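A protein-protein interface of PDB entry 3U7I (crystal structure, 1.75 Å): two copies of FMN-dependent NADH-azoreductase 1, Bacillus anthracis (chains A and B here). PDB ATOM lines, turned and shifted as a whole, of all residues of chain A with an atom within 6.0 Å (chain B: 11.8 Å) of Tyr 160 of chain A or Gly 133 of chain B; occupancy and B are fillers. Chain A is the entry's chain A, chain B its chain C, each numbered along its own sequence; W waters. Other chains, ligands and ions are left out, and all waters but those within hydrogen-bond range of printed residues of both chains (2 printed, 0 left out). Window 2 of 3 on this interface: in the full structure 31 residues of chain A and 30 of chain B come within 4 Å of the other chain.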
ATOM      1  N   PHE A 107     -27.516 -15.786  -5.991  1.00  0.00           N
ATOM      2  CA  PHE A 107     -28.287 -14.927  -5.072  1.00  0.00           C
ATOM      3  C   PHE A 107     -29.709 -15.379  -4.698  1.00  0.00           C
ATOM      4  O   PHE A 107     -30.560 -14.547  -4.414  1.00  0.00           O
ATOM      5  CB  PHE A 107     -28.300 -13.489  -5.591  1.00  0.00           C
ATOM      6  CG  PHE A 107     -26.931 -12.976  -5.939  1.00  0.00           C
ATOM      7  CD1 PHE A 107     -26.036 -12.623  -4.940  1.00  0.00           C
ATOM      8  CD2 PHE A 107     -26.529 -12.876  -7.268  1.00  0.00           C
ATOM      9  CE1 PHE A 107     -24.771 -12.165  -5.252  1.00  0.00           C
ATOM     10  CE2 PHE A 107     -25.256 -12.418  -7.592  1.00  0.00           C
ATOM     11  CZ  PHE A 107     -24.377 -12.059  -6.584  1.00  0.00           C
ATOM     12  N   GLY A 152     -19.076 -14.494  -1.844  1.00  0.00           N
ATOM     13  CA  GLY A 152     -19.076 -13.121  -1.377  1.00  0.00           C
ATOM     14  C   GLY A 152     -19.355 -13.021   0.109  1.00  0.00           C
ATOM     15  O   GLY A 152     -19.730 -14.012   0.756  1.00  0.00           O
ATOM     16  N   ILE A 153     -19.164 -11.822   0.651  1.00  0.00           N
ATOM     17  CA  ILE A 153     -19.419 -11.560   2.062  1.00  0.00           C
ATOM     18  C   ILE A 153     -20.701 -10.736   2.170  1.00  0.00           C
ATOM     19  O   ILE A 153     -20.864  -9.737   1.464  1.00  0.00           O
ATOM     20  CB  ILE A 153     -18.207 -10.843   2.728  1.00  0.00           C
ATOM     21  CG1 ILE A 153     -17.036 -11.825   2.888  1.00  0.00           C
ATOM     22  CG2 ILE A 153     -18.588 -10.254   4.086  1.00  0.00           C
ATOM     23  CD1 ILE A 153     -15.707 -11.162   3.201  1.00  0.00           C
ATOM     24  N   TYR A 154     -21.611 -11.163   3.044  1.00  0.00           N
ATOM     25  CA  TYR A 154     -22.975 -10.614   3.067  1.00  0.00           C
ATOM     26  C   TYR A 154     -23.304  -9.764   4.292  1.00  0.00           C
ATOM     27  O   TYR A 154     -24.413  -9.231   4.414  1.00  0.00           O
ATOM     28  CB  TYR A 154     -24.009 -11.744   2.869  1.00  0.00           C
ATOM     29  CG  TYR A 154     -23.976 -12.233   1.443  1.00  0.00           C
ATOM     30  CD1 TYR A 154     -24.898 -11.775   0.512  1.00  0.00           C
ATOM     31  CD2 TYR A 154     -22.972 -13.095   1.004  1.00  0.00           C
ATOM     32  CE1 TYR A 154     -24.848 -12.194  -0.806  1.00  0.00           C
ATOM     33  CE2 TYR A 154     -22.912 -13.512  -0.317  1.00  0.00           C
ATOM     34  CZ  TYR A 154     -23.855 -13.053  -1.216  1.00  0.00           C
ATOM     35  OH  TYR A 154     -23.807 -13.460  -2.530  1.00  0.00           O
ATOM     36  N   ASP A 158     -24.101  -3.865   2.345  1.00  0.00           N
ATOM     37  CA  ASP A 158     -23.883  -3.266   1.038  1.00  0.00           C
ATOM     38  C   ASP A 158     -24.735  -4.041   0.025  1.00  0.00           C
ATOM     39  O   ASP A 158     -25.685  -4.730   0.407  1.00  0.00           O
ATOM     40  CB  ASP A 158     -22.404  -3.338   0.677  1.00  0.00           C
ATOM     41  CG  ASP A 158     -21.851  -4.754   0.768  1.00  0.00           C
ATOM     42  OD1 ASP A 158     -22.646  -5.720   0.784  1.00  0.00           O
ATOM     43  OD2 ASP A 158     -20.615  -4.902   0.812  1.00  0.00           O
ATOM     44  N   TRP A 159     -24.401  -3.935  -1.255  1.00  0.00           N
ATOM     45  CA  TRP A 159     -25.191  -4.577  -2.305  1.00  0.00           C
ATOM     46  C   TRP A 159     -25.427  -6.059  -2.017  1.00  0.00           C
ATOM     47  O   TRP A 159     -26.537  -6.556  -2.195  1.00  0.00           O
ATOM     48  CB  TRP A 159     -24.526  -4.381  -3.676  1.00  0.00           C
ATOM     49  CG  TRP A 159     -25.237  -5.062  -4.835  1.00  0.00           C
ATOM     50  CD1 TRP A 159     -26.313  -4.589  -5.529  1.00  0.00           C
ATOM     51  CD2 TRP A 159     -24.896  -6.322  -5.439  1.00  0.00           C
ATOM     52  NE1 TRP A 159     -26.672  -5.478  -6.515  1.00  0.00           N
ATOM     53  CE2 TRP A 159     -25.821  -6.544  -6.484  1.00  0.00           C
ATOM     54  CE3 TRP A 159     -23.911  -7.283  -5.190  1.00  0.00           C
ATOM     55  CZ2 TRP A 159     -25.779  -7.696  -7.286  1.00  0.00           C
ATOM     56  CZ3 TRP A 159     -23.880  -8.426  -5.984  1.00  0.00           C
ATOM     57  CH2 TRP A 159     -24.805  -8.616  -7.020  1.00  0.00           C
ATOM     58  N   TYR A 160     -24.390  -6.760  -1.564  1.00  0.00           N
ATOM     59  CA  TYR A 160     -24.513  -8.190  -1.251  1.00  0.00           C
ATOM     60  C   TYR A 160     -25.603  -8.468  -0.214  1.00  0.00           C
ATOM     61  O   TYR A 160     -26.367  -9.426  -0.350  1.00  0.00           O
ATOM     62  CB  TYR A 160     -23.161  -8.788  -0.829  1.00  0.00           C
ATOM     63  CG  TYR A 160     -22.170  -8.858  -1.979  1.00  0.00           C
ATOM     64  CD1 TYR A 160     -22.143  -9.958  -2.841  1.00  0.00           C
ATOM     65  CD2 TYR A 160     -21.283  -7.813  -2.219  1.00  0.00           C
ATOM     66  CE1 TYR A 160     -21.248 -10.018  -3.897  1.00  0.00           C
ATOM     67  CE2 TYR A 160     -20.383  -7.862  -3.275  1.00  0.00           C
ATOM     68  CZ  TYR A 160     -20.367  -8.965  -4.112  1.00  0.00           C
ATOM     69  OH  TYR A 160     -19.469  -8.999  -5.166  1.00  0.00           O
ATOM     70  N   THR A 161     -25.692  -7.622   0.810  1.00  0.00           N
ATOM     71  CA  THR A 161     -26.736  -7.792   1.820  1.00  0.00           C
ATOM     72  C   THR A 161     -28.122  -7.625   1.182  1.00  0.00           C
ATOM     73  O   THR A 161     -29.065  -8.373   1.494  1.00  0.00           O
ATOM     74  CB  THR A 161     -26.571  -6.801   2.982  1.00  0.00           C
ATOM     75  OG1 THR A 161     -25.193  -6.750   3.381  1.00  0.00           O
ATOM     76  CG2 THR A 161     -27.422  -7.244   4.165  1.00  0.00           C
ATOM     77  N   ASP A 162     -28.224  -6.660   0.269  1.00  0.00           N
ATOM     78  CA  ASP A 162     -29.480  -6.347  -0.419  1.00  0.00           C
ATOM     79  C   ASP A 162     -29.972  -7.447  -1.373  1.00  0.00           C
ATOM     80  O   ASP A 162     -31.171  -7.524  -1.653  1.00  0.00           O
ATOM     81  CB  ASP A 162     -29.359  -5.032  -1.198  1.00  0.00           C
ATOM     82  CG  ASP A 162     -29.303  -3.805  -0.292  1.00  0.00           C
ATOM     83  OD1 ASP A 162     -29.837  -3.852   0.838  1.00  0.00           O
ATOM     84  OD2 ASP A 162     -28.728  -2.782  -0.729  1.00  0.00           O
ATOM     85  N   VAL A 163     -29.059  -8.275  -1.884  1.00  0.00           N
ATOM     86  CA  VAL A 163     -29.443  -9.347  -2.819  1.00  0.00           C
ATOM     87  C   VAL A 163     -29.318 -10.759  -2.234  1.00  0.00           C
ATOM     88  O   VAL A 163     -29.299 -11.743  -2.969  1.00  0.00           O
ATOM     89  CB  VAL A 163     -28.642  -9.285  -4.135  1.00  0.00           C
ATOM     90  CG1 VAL A 163     -28.934  -7.977  -4.883  1.00  0.00           C
ATOM     91  CG2 VAL A 163     -27.145  -9.459  -3.860  1.00  0.00           C
ATOM     92  N   GLU A 164     -29.251 -10.864  -0.913  1.00  0.00           N
ATOM     93  CA  GLU A 164     -29.148 -12.173  -0.294  1.00  0.00           C
ATOM     94  C   GLU A 164     -30.528 -12.822  -0.184  1.00  0.00           C
ATOM     95  O   GLU A 164     -31.016 -13.095   0.917  1.00  0.00           O
ATOM     96  CB  GLU A 164     -28.475 -12.077   1.081  1.00  0.00           C
ATOM     97  CG  GLU A 164     -27.913 -13.427   1.575  1.00  0.00           C
ATOM     98  CD  GLU A 164     -27.488 -13.408   3.045  1.00  0.00           C
ATOM     99  OE1 GLU A 164     -27.827 -12.437   3.771  1.00  0.00           O
ATOM    100  OE2 GLU A 164     -26.818 -14.377   3.475  1.00  0.00           O
ATOM    101  N   MET B 121     -26.663 -16.345 -16.182  1.00  0.00           N
ATOM    102  CA  MET B 121     -25.722 -15.550 -15.378  1.00  0.00           C
ATOM    103  C   MET B 121     -24.351 -16.210 -15.375  1.00  0.00           C
ATOM    104  O   MET B 121     -24.060 -17.065 -14.525  1.00  0.00           O
ATOM    105  CB  MET B 121     -26.227 -15.332 -13.951  1.00  0.00           C
ATOM    106  CG  MET B 121     -27.414 -14.390 -13.876  1.00  0.00           C
ATOM    107  SD  MET B 121     -28.005 -14.164 -12.070  1.00  0.00           S
ATOM    108  CE  MET B 121     -26.406 -13.304 -11.346  1.00  0.00           C
ATOM    109  N   ALA B 123     -20.047 -15.648 -15.950  1.00  0.00           N
ATOM    110  CA  ALA B 123     -18.926 -14.709 -15.906  1.00  0.00           C
ATOM    111  C   ALA B 123     -18.252 -14.598 -17.272  1.00  0.00           C
ATOM    112  O   ALA B 123     -18.150 -15.583 -18.012  1.00  0.00           O
ATOM    113  CB  ALA B 123     -17.918 -15.115 -14.834  1.00  0.00           C
ATOM    114  N   ARG B 124     -17.797 -13.394 -17.601  1.00  0.00           N
ATOM    115  CA  ARG B 124     -17.173 -13.132 -18.895  1.00  0.00           C
ATOM    116  C   ARG B 124     -18.192 -13.099 -20.043  1.00  0.00           C
ATOM    117  O   ARG B 124     -17.831 -12.817 -21.194  1.00  0.00           O
ATOM    118  CB  ARG B 124     -16.060 -14.157 -19.175  1.00  0.00           C
ATOM    119  CG  ARG B 124     -14.746 -13.898 -18.416  1.00  0.00           C
ATOM    120  CD  ARG B 124     -13.886 -15.156 -18.293  1.00  0.00           C
ATOM    121  NE  ARG B 124     -13.655 -15.799 -19.585  1.00  0.00           N
ATOM    122  CZ  ARG B 124     -13.693 -17.116 -19.785  1.00  0.00           C
ATOM    123  NH1 ARG B 124     -13.473 -17.614 -20.998  1.00  0.00           N
ATOM    124  NH2 ARG B 124     -13.950 -17.937 -18.775  1.00  0.00           N
ATOM    125  N   THR B 126     -22.350 -12.497 -19.339  1.00  0.00           N
ATOM    126  CA  THR B 126     -23.377 -11.499 -19.011  1.00  0.00           C
ATOM    127  C   THR B 126     -22.960 -10.593 -17.845  1.00  0.00           C
ATOM    128  O   THR B 126     -23.579  -9.553 -17.591  1.00  0.00           O
ATOM    129  CB  THR B 126     -24.753 -12.149 -18.758  1.00  0.00           C
ATOM    130  OG1 THR B 126     -24.648 -13.074 -17.674  1.00  0.00           O
ATOM    131  CG2 THR B 126     -25.228 -12.900 -20.016  1.00  0.00           C
ATOM    132  N   PHE B 127     -21.900 -10.994 -17.146  1.00  0.00           N
ATOM    133  CA  PHE B 127     -21.299 -10.179 -16.093  1.00  0.00           C
ATOM    134  C   PHE B 127     -19.814 -10.518 -15.973  1.00  0.00           C
ATOM    135  O   PHE B 127     -19.349 -11.525 -16.519  1.00  0.00           O
ATOM    136  CB  PHE B 127     -22.015 -10.388 -14.742  1.00  0.00           C
ATOM    137  CG  PHE B 127     -21.596 -11.640 -14.004  1.00  0.00           C
ATOM    138  CD1 PHE B 127     -20.490 -11.628 -13.157  1.00  0.00           C
ATOM    139  CD2 PHE B 127     -22.320 -12.820 -14.140  1.00  0.00           C
ATOM    140  CE1 PHE B 127     -20.098 -12.777 -12.478  1.00  0.00           C
ATOM    141  CE2 PHE B 127     -21.938 -13.975 -13.455  1.00  0.00           C
ATOM    142  CZ  PHE B 127     -20.825 -13.954 -12.629  1.00  0.00           C
ATOM    143  N   LYS B 128     -19.067  -9.678 -15.266  1.00  0.00           N
ATOM    144  CA  LYS B 128     -17.670  -9.992 -15.011  1.00  0.00           C
ATOM    145  C   LYS B 128     -17.253  -9.612 -13.599  1.00  0.00           C
ATOM    146  O   LYS B 128     -17.815  -8.696 -12.997  1.00  0.00           O
ATOM    147  CB  LYS B 128     -16.751  -9.327 -16.042  1.00  0.00           C
ATOM    148  CG  LYS B 128     -16.609  -7.825 -15.891  1.00  0.00           C
ATOM    149  CD  LYS B 128     -15.405  -7.335 -16.672  1.00  0.00           C
ATOM    150  CE  LYS B 128     -15.319  -5.825 -16.672  1.00  0.00           C
ATOM    151  NZ  LYS B 128     -13.990  -5.355 -17.145  1.00  0.00           N
ATOM    152  N   TYR B 129     -16.275 -10.340 -13.072  1.00  0.00           N
ATOM    153  CA  TYR B 129     -15.700 -10.024 -11.774  1.00  0.00           C
ATOM    154  C   TYR B 129     -14.645  -8.933 -11.916  1.00  0.00           C
ATOM    155  O   TYR B 129     -13.887  -8.916 -12.886  1.00  0.00           O
ATOM    156  CB  TYR B 129     -15.098 -11.275 -11.140  1.00  0.00           C
ATOM    157  CG  TYR B 129     -16.121 -12.342 -10.837  1.00  0.00           C
ATOM    158  CD1 TYR B 129     -17.053 -12.168  -9.822  1.00  0.00           C
ATOM    159  CD2 TYR B 129     -16.153 -13.526 -11.558  1.00  0.00           C
ATOM    160  CE1 TYR B 129     -17.998 -13.150  -9.535  1.00  0.00           C
ATOM    161  CE2 TYR B 129     -17.091 -14.516 -11.278  1.00  0.00           C
ATOM    162  CZ  TYR B 129     -18.012 -14.324 -10.264  1.00  0.00           C
ATOM    163  OH  TYR B 129     -18.947 -15.301  -9.979  1.00  0.00           O
ATOM    164  N   THR B 130     -14.625  -8.012 -10.952  1.00  0.00           N
ATOM    165  CA  THR B 130     -13.606  -6.967 -10.876  1.00  0.00           C
ATOM    166  C   THR B 130     -12.975  -6.999  -9.485  1.00  0.00           C
ATOM    167  O   THR B 130     -13.040  -8.022  -8.797  1.00  0.00           O
ATOM    168  CB  THR B 130     -14.190  -5.563 -11.166  1.00  0.00           C
ATOM    169  OG1 THR B 130     -15.101  -5.185 -10.126  1.00  0.00           O
ATOM    170  CG2 THR B 130     -14.918  -5.552 -12.502  1.00  0.00           C
ATOM    171  N   GLU B 131     -12.378  -5.885  -9.067  1.00  0.00           N
ATOM    172  CA  GLU B 131     -11.709  -5.809  -7.765  1.00  0.00           C
ATOM    173  C   GLU B 131     -12.655  -5.403  -6.637  1.00  0.00           C
ATOM    174  O   GLU B 131     -12.560  -5.913  -5.521  1.00  0.00           O
ATOM    175  CB  GLU B 131     -10.531  -4.838  -7.825  1.00  0.00           C
ATOM    176  CG  GLU B 131      -9.461  -5.241  -8.822  1.00  0.00           C
ATOM    177  CD  GLU B 131      -8.656  -4.057  -9.313  1.00  0.00           C
ATOM    178  OE1 GLU B 131      -8.867  -3.633 -10.471  1.00  0.00           O
ATOM    179  OE2 GLU B 131      -7.810  -3.548  -8.543  1.00  0.00           O
ATOM    180  N   THR B 132     -13.564  -4.481  -6.934  1.00  0.00           N
ATOM    181  CA  THR B 132     -14.527  -4.009  -5.947  1.00  0.00           C
ATOM    182  C   THR B 132     -15.846  -4.781  -6.029  1.00  0.00           C
ATOM    183  O   THR B 132     -16.896  -4.282  -5.618  1.00  0.00           O
ATOM    184  CB  THR B 132     -14.798  -2.505  -6.116  1.00  0.00           C
ATOM    185  OG1 THR B 132     -15.160  -2.238  -7.477  1.00  0.00           O
ATOM    186  CG2 THR B 132     -13.556  -1.697  -5.764  1.00  0.00           C
ATOM    187  N   GLY B 133     -15.780  -5.999  -6.561  1.00  0.00           N
ATOM    188  CA  GLY B 133     -16.950  -6.855  -6.687  1.00  0.00           C
ATOM    189  C   GLY B 133     -17.126  -7.434  -8.083  1.00  0.00           C
ATOM    190  O   GLY B 133     -16.287  -8.205  -8.557  1.00  0.00           O
ATOM    191  N   SER B 134     -18.231  -7.070  -8.732  1.00  0.00           N
ATOM    192  CA  SER B 134     -18.491  -7.456 -10.118  1.00  0.00           C
ATOM    193  C   SER B 134     -19.386  -6.424 -10.799  1.00  0.00           C
ATOM    194  O   SER B 134     -19.897  -5.504 -10.158  1.00  0.00           O
ATOM    195  CB  SER B 134     -19.111  -8.853 -10.205  1.00  0.00           C
ATOM    196  OG  SER B 134     -20.269  -8.953  -9.401  1.00  0.00           O
ATOM    197  N   VAL B 135     -19.558  -6.578 -12.108  1.00  0.00           N
ATOM    198  CA  VAL B 135     -20.362  -5.649 -12.894  1.00  0.00           C
ATOM    199  C   VAL B 135     -21.059  -6.399 -14.036  1.00  0.00           C
ATOM    200  O   VAL B 135     -20.556  -7.419 -14.514  1.00  0.00           O
ATOM    201  CB  VAL B 135     -19.510  -4.450 -13.424  1.00  0.00           C
ATOM    202  CG1 VAL B 135     -18.376  -4.929 -14.317  1.00  0.00           C
ATOM    203  CG2 VAL B 135     -20.381  -3.429 -14.150  1.00  0.00           C
ATOM    204  N   GLY B 136     -22.229  -5.909 -14.445  1.00  0.00           N
ATOM    205  CA  GLY B 136     -22.975  -6.509 -15.540  1.00  0.00           C
ATOM    206  C   GLY B 136     -22.407  -6.090 -16.884  1.00  0.00           C
ATOM    207  O   GLY B 136     -21.873  -4.983 -17.020  1.00  0.00           O
ATOM    208  N   LEU B 137     -22.516  -6.980 -17.873  1.00  0.00           N
ATOM    209  CA  LEU B 137     -21.968  -6.735 -19.206  1.00  0.00           C
ATOM    210  C   LEU B 137     -23.029  -6.370 -20.244  1.00  0.00           C
ATOM    211  O   LEU B 137     -22.698  -6.041 -21.381  1.00  0.00           O
ATOM    212  CB  LEU B 137     -21.171  -7.954 -19.682  1.00  0.00           C
ATOM    213  CG  LEU B 137     -19.922  -8.270 -18.871  1.00  0.00           C
ATOM    214  CD1 LEU B 137     -19.160  -9.398 -19.517  1.00  0.00           C
ATOM    215  CD2 LEU B 137     -19.050  -7.023 -18.757  1.00  0.00           C
ATOM    216  N   LYS B 139     -25.124  -3.731 -20.437  1.00  0.00           N
ATOM    217  CA  LYS B 139     -25.561  -2.375 -20.132  1.00  0.00           C
ATOM    218  C   LYS B 139     -25.783  -1.582 -21.418  1.00  0.00           C
ATOM    219  O   LYS B 139     -25.180  -0.534 -21.614  1.00  0.00           O
ATOM    220  CB  LYS B 139     -24.530  -1.670 -19.243  1.00  0.00           C
ATOM    221  CG  LYS B 139     -24.057  -2.519 -18.067  1.00  0.00           C
ATOM    222  CD  LYS B 139     -23.813  -1.688 -16.817  1.00  0.00           C
ATOM    223  CE  LYS B 139     -23.478  -2.584 -15.627  1.00  0.00           C
ATOM    224  NZ  LYS B 139     -24.199  -2.190 -14.379  1.00  0.00           N
ATOM    225  N   TYR B 165     -40.702 -12.101  -3.416  1.00  0.00           N
ATOM    226  CA  TYR B 165     -39.310 -12.326  -3.801  1.00  0.00           C
ATOM    227  C   TYR B 165     -39.124 -12.684  -5.264  1.00  0.00           C
ATOM    228  O   TYR B 165     -38.043 -12.496  -5.809  1.00  0.00           O
ATOM    229  CB  TYR B 165     -38.633 -13.344  -2.882  1.00  0.00           C
ATOM    230  CG  TYR B 165     -38.442 -12.791  -1.496  1.00  0.00           C
ATOM    231  CD1 TYR B 165     -37.617 -11.687  -1.283  1.00  0.00           C
ATOM    232  CD2 TYR B 165     -39.104 -13.344  -0.401  1.00  0.00           C
ATOM    233  CE1 TYR B 165     -37.445 -11.157  -0.023  1.00  0.00           C
ATOM    234  CE2 TYR B 165     -38.936 -12.817   0.868  1.00  0.00           C
ATOM    235  CZ  TYR B 165     -38.097 -11.729   1.047  1.00  0.00           C
ATOM    236  OH  TYR B 165     -37.925 -11.198   2.303  1.00  0.00           O
ATOM    237  N   LYS B 168     -38.750  -9.074  -6.536  1.00  0.00           N
ATOM    238  CA  LYS B 168     -37.539  -8.498  -5.955  1.00  0.00           C
ATOM    239  C   LYS B 168     -36.285  -9.103  -6.583  1.00  0.00           C
ATOM    240  O   LYS B 168     -35.370  -8.384  -6.997  1.00  0.00           O
ATOM    241  CB  LYS B 168     -37.538  -8.677  -4.430  1.00  0.00           C
ATOM    242  CG  LYS B 168     -38.564  -7.794  -3.743  1.00  0.00           C
ATOM    243  CD  LYS B 168     -38.511  -7.933  -2.232  1.00  0.00           C
ATOM    244  CE  LYS B 168     -39.295  -6.807  -1.560  1.00  0.00           C
ATOM    245  NZ  LYS B 168     -39.032  -6.793  -0.094  1.00  0.00           N
ATOM    246  N   TYR B 169     -36.260 -10.426  -6.678  1.00  0.00           N
ATOM    247  CA  TYR B 169     -35.119 -11.122  -7.249  1.00  0.00           C
ATOM    248  C   TYR B 169     -34.939 -10.787  -8.725  1.00  0.00           C
ATOM    249  O   TYR B 169     -33.849 -10.389  -9.144  1.00  0.00           O
ATOM    250  CB  TYR B 169     -35.274 -12.625  -7.063  1.00  0.00           C
ATOM    251  CG  TYR B 169     -34.175 -13.444  -7.682  1.00  0.00           C
ATOM    252  CD1 TYR B 169     -32.931 -13.537  -7.075  1.00  0.00           C
ATOM    253  CD2 TYR B 169     -34.380 -14.131  -8.868  1.00  0.00           C
ATOM    254  CE1 TYR B 169     -31.921 -14.293  -7.630  1.00  0.00           C
ATOM    255  CE2 TYR B 169     -33.375 -14.889  -9.437  1.00  0.00           C
ATOM    256  CZ  TYR B 169     -32.145 -14.972  -8.817  1.00  0.00           C
ATOM    257  OH  TYR B 169     -31.136 -15.740  -9.369  1.00  0.00           O
ATOM    258  N   ALA B 172     -33.749  -7.183  -9.352  1.00  0.00           N
ATOM    259  CA  ALA B 172     -32.377  -7.078  -8.842  1.00  0.00           C
ATOM    260  C   ALA B 172     -31.350  -7.691  -9.791  1.00  0.00           C
ATOM    261  O   ALA B 172     -30.354  -7.037 -10.144  1.00  0.00           O
ATOM    262  CB  ALA B 172     -32.266  -7.721  -7.447  1.00  0.00           C
ATOM    263  N   MET B 173     -31.591  -8.944 -10.193  1.00  0.00           N
ATOM    264  CA  MET B 173     -30.658  -9.668 -11.049  1.00  0.00           C
ATOM    265  C   MET B 173     -30.519  -8.963 -12.389  1.00  0.00           C
ATOM    266  O   MET B 173     -29.407  -8.754 -12.886  1.00  0.00           O
ATOM    267  CB  MET B 173     -31.110 -11.107 -11.266  1.00  0.00           C
ATOM    268  CG  MET B 173     -31.057 -11.956  -9.999  1.00  0.00           C
ATOM    269  SD  MET B 173     -29.299 -12.003  -9.147  1.00  0.00           S
ATOM    270  CE  MET B 173     -29.600 -10.732  -7.711  1.00  0.00           C
ATOM    271  N   ASN B 175     -31.182  -5.855 -13.176  1.00  0.00           N
ATOM    272  CA  ASN B 175     -30.520  -4.561 -12.997  1.00  0.00           C
ATOM    273  C   ASN B 175     -29.012  -4.751 -12.860  1.00  0.00           C
ATOM    274  O   ASN B 175     -28.207  -4.003 -13.435  1.00  0.00           O
ATOM    275  CB  ASN B 175     -31.073  -3.788 -11.803  1.00  0.00           C
ATOM    276  CG  ASN B 175     -30.527  -2.368 -11.741  1.00  0.00           C
ATOM    277  OD1 ASN B 175     -31.135  -1.432 -12.269  1.00  0.00           O
ATOM    278  ND2 ASN B 175     -29.372  -2.204 -11.104  1.00  0.00           N
ATOM    279  N   PHE B 176     -28.638  -5.777 -12.104  1.00  0.00           N
ATOM    280  CA  PHE B 176     -27.239  -6.161 -11.997  1.00  0.00           C
ATOM    281  C   PHE B 176     -26.610  -6.416 -13.375  1.00  0.00           C
ATOM    282  O   PHE B 176     -25.537  -5.895 -13.676  1.00  0.00           O
ATOM    283  CB  PHE B 176     -27.088  -7.385 -11.096  1.00  0.00           C
ATOM    284  CG  PHE B 176     -25.721  -7.984 -11.126  1.00  0.00           C
ATOM    285  CD1 PHE B 176     -24.620  -7.244 -10.716  1.00  0.00           C
ATOM    286  CD2 PHE B 176     -25.535  -9.290 -11.559  1.00  0.00           C
ATOM    287  CE1 PHE B 176     -23.347  -7.795 -10.740  1.00  0.00           C
ATOM    288  CE2 PHE B 176     -24.267  -9.848 -11.587  1.00  0.00           C
ATOM    289  CZ  PHE B 176     -23.171  -9.096 -11.179  1.00  0.00           C
HETATM  290  O   HOH W   1     -20.123 -10.754  -6.947  1.00  0.00           O
HETATM  291  O   HOH W   2     -29.041  -5.269  -8.479  1.00  0.00           O
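The backbone carbonyl oxygen (O) of Phe 176 of chain B sits close to the backbone NH (N) of Gly 136 of chain B. The side-chain carboxylate (OD1) of Asp 158 of chain A is in hydrogen-bond range of the backbone NH (N) of Tyr 160 of chain A.
Phe 107 of chain A touches Tyr 169 of chain B. Met 173 of chain B touches Phe 107 of chain A. Trp 159 of chain A touches Phe 176 of chain B (CZ2 to CD1, 3.6 Å). Gly 133 of chain B touches Tyr 160 of chain A. CB of Val 163 of chain A touches CE of Met 173 of chain B (3.97 Å).
Of chain B, only Gly 133 (3.6 Å) comes within 4 Å of Tyr 160 of chain A. No residue of chain B comes within 4 Å of Tyr 154 of chain A. Thr 161 of chain A touches none of the printed residues of chain B. No residue of chain B comes within 4 Å of Asp 162 of chain A. Glu 164 of chain A touches none of the printed residues of chain B. Printed residues of chain A within 4 Å of Phe 176 of chain B: Trp 159 (3.6 Å). Of the printed residues of chain B, Phe 107 of chain A touches Tyr 169 (3.5 Å) and Met 173 (3.5 Å). Of the printed residues of chain A, Met 173 of chain B touches Phe 107 (3.5 Å) and Val 163 (3.97 Å). Printed residues of chain A within 4 Å of Tyr 169 of chain B: Phe 107 (3.5 Å). The nearest printed residue of chain A that does not touch Gly 133 of chain B is Trp 159 of chain A (7.1 Å).
Hydrophobic or aromatic side chains of chain A that line the printed part of chain B: Phe 107, Trp 159, Tyr 160 and Val 163. Along chain A the printed residues that touch a printed residue of chain B span positions 107 to 163. Among the printed residues, 5 pairs touch across the chains. Among the printed residues, no Asp or Glu carboxylate lies within 4 Å of a Lys or Arg side-chain nitrogen of the other chain.
No position is printed for both chains. Of the 5 pairs that touch across the chains among the printed residues, none has its exchanged pair printed and touching as well.
Water W1 bridges the side-chain hydroxyl of Tyr 160 of chain A (2.6 Å) and the side-chain hydroxyl of Ser 134 of chain B (3.0 Å). Water W2 bridges the backbone carbonyl oxygen of Ala 172 of chain B (2.8 Å) and the indole nitrogen of Trp 159 of chain A (3.1 Å).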
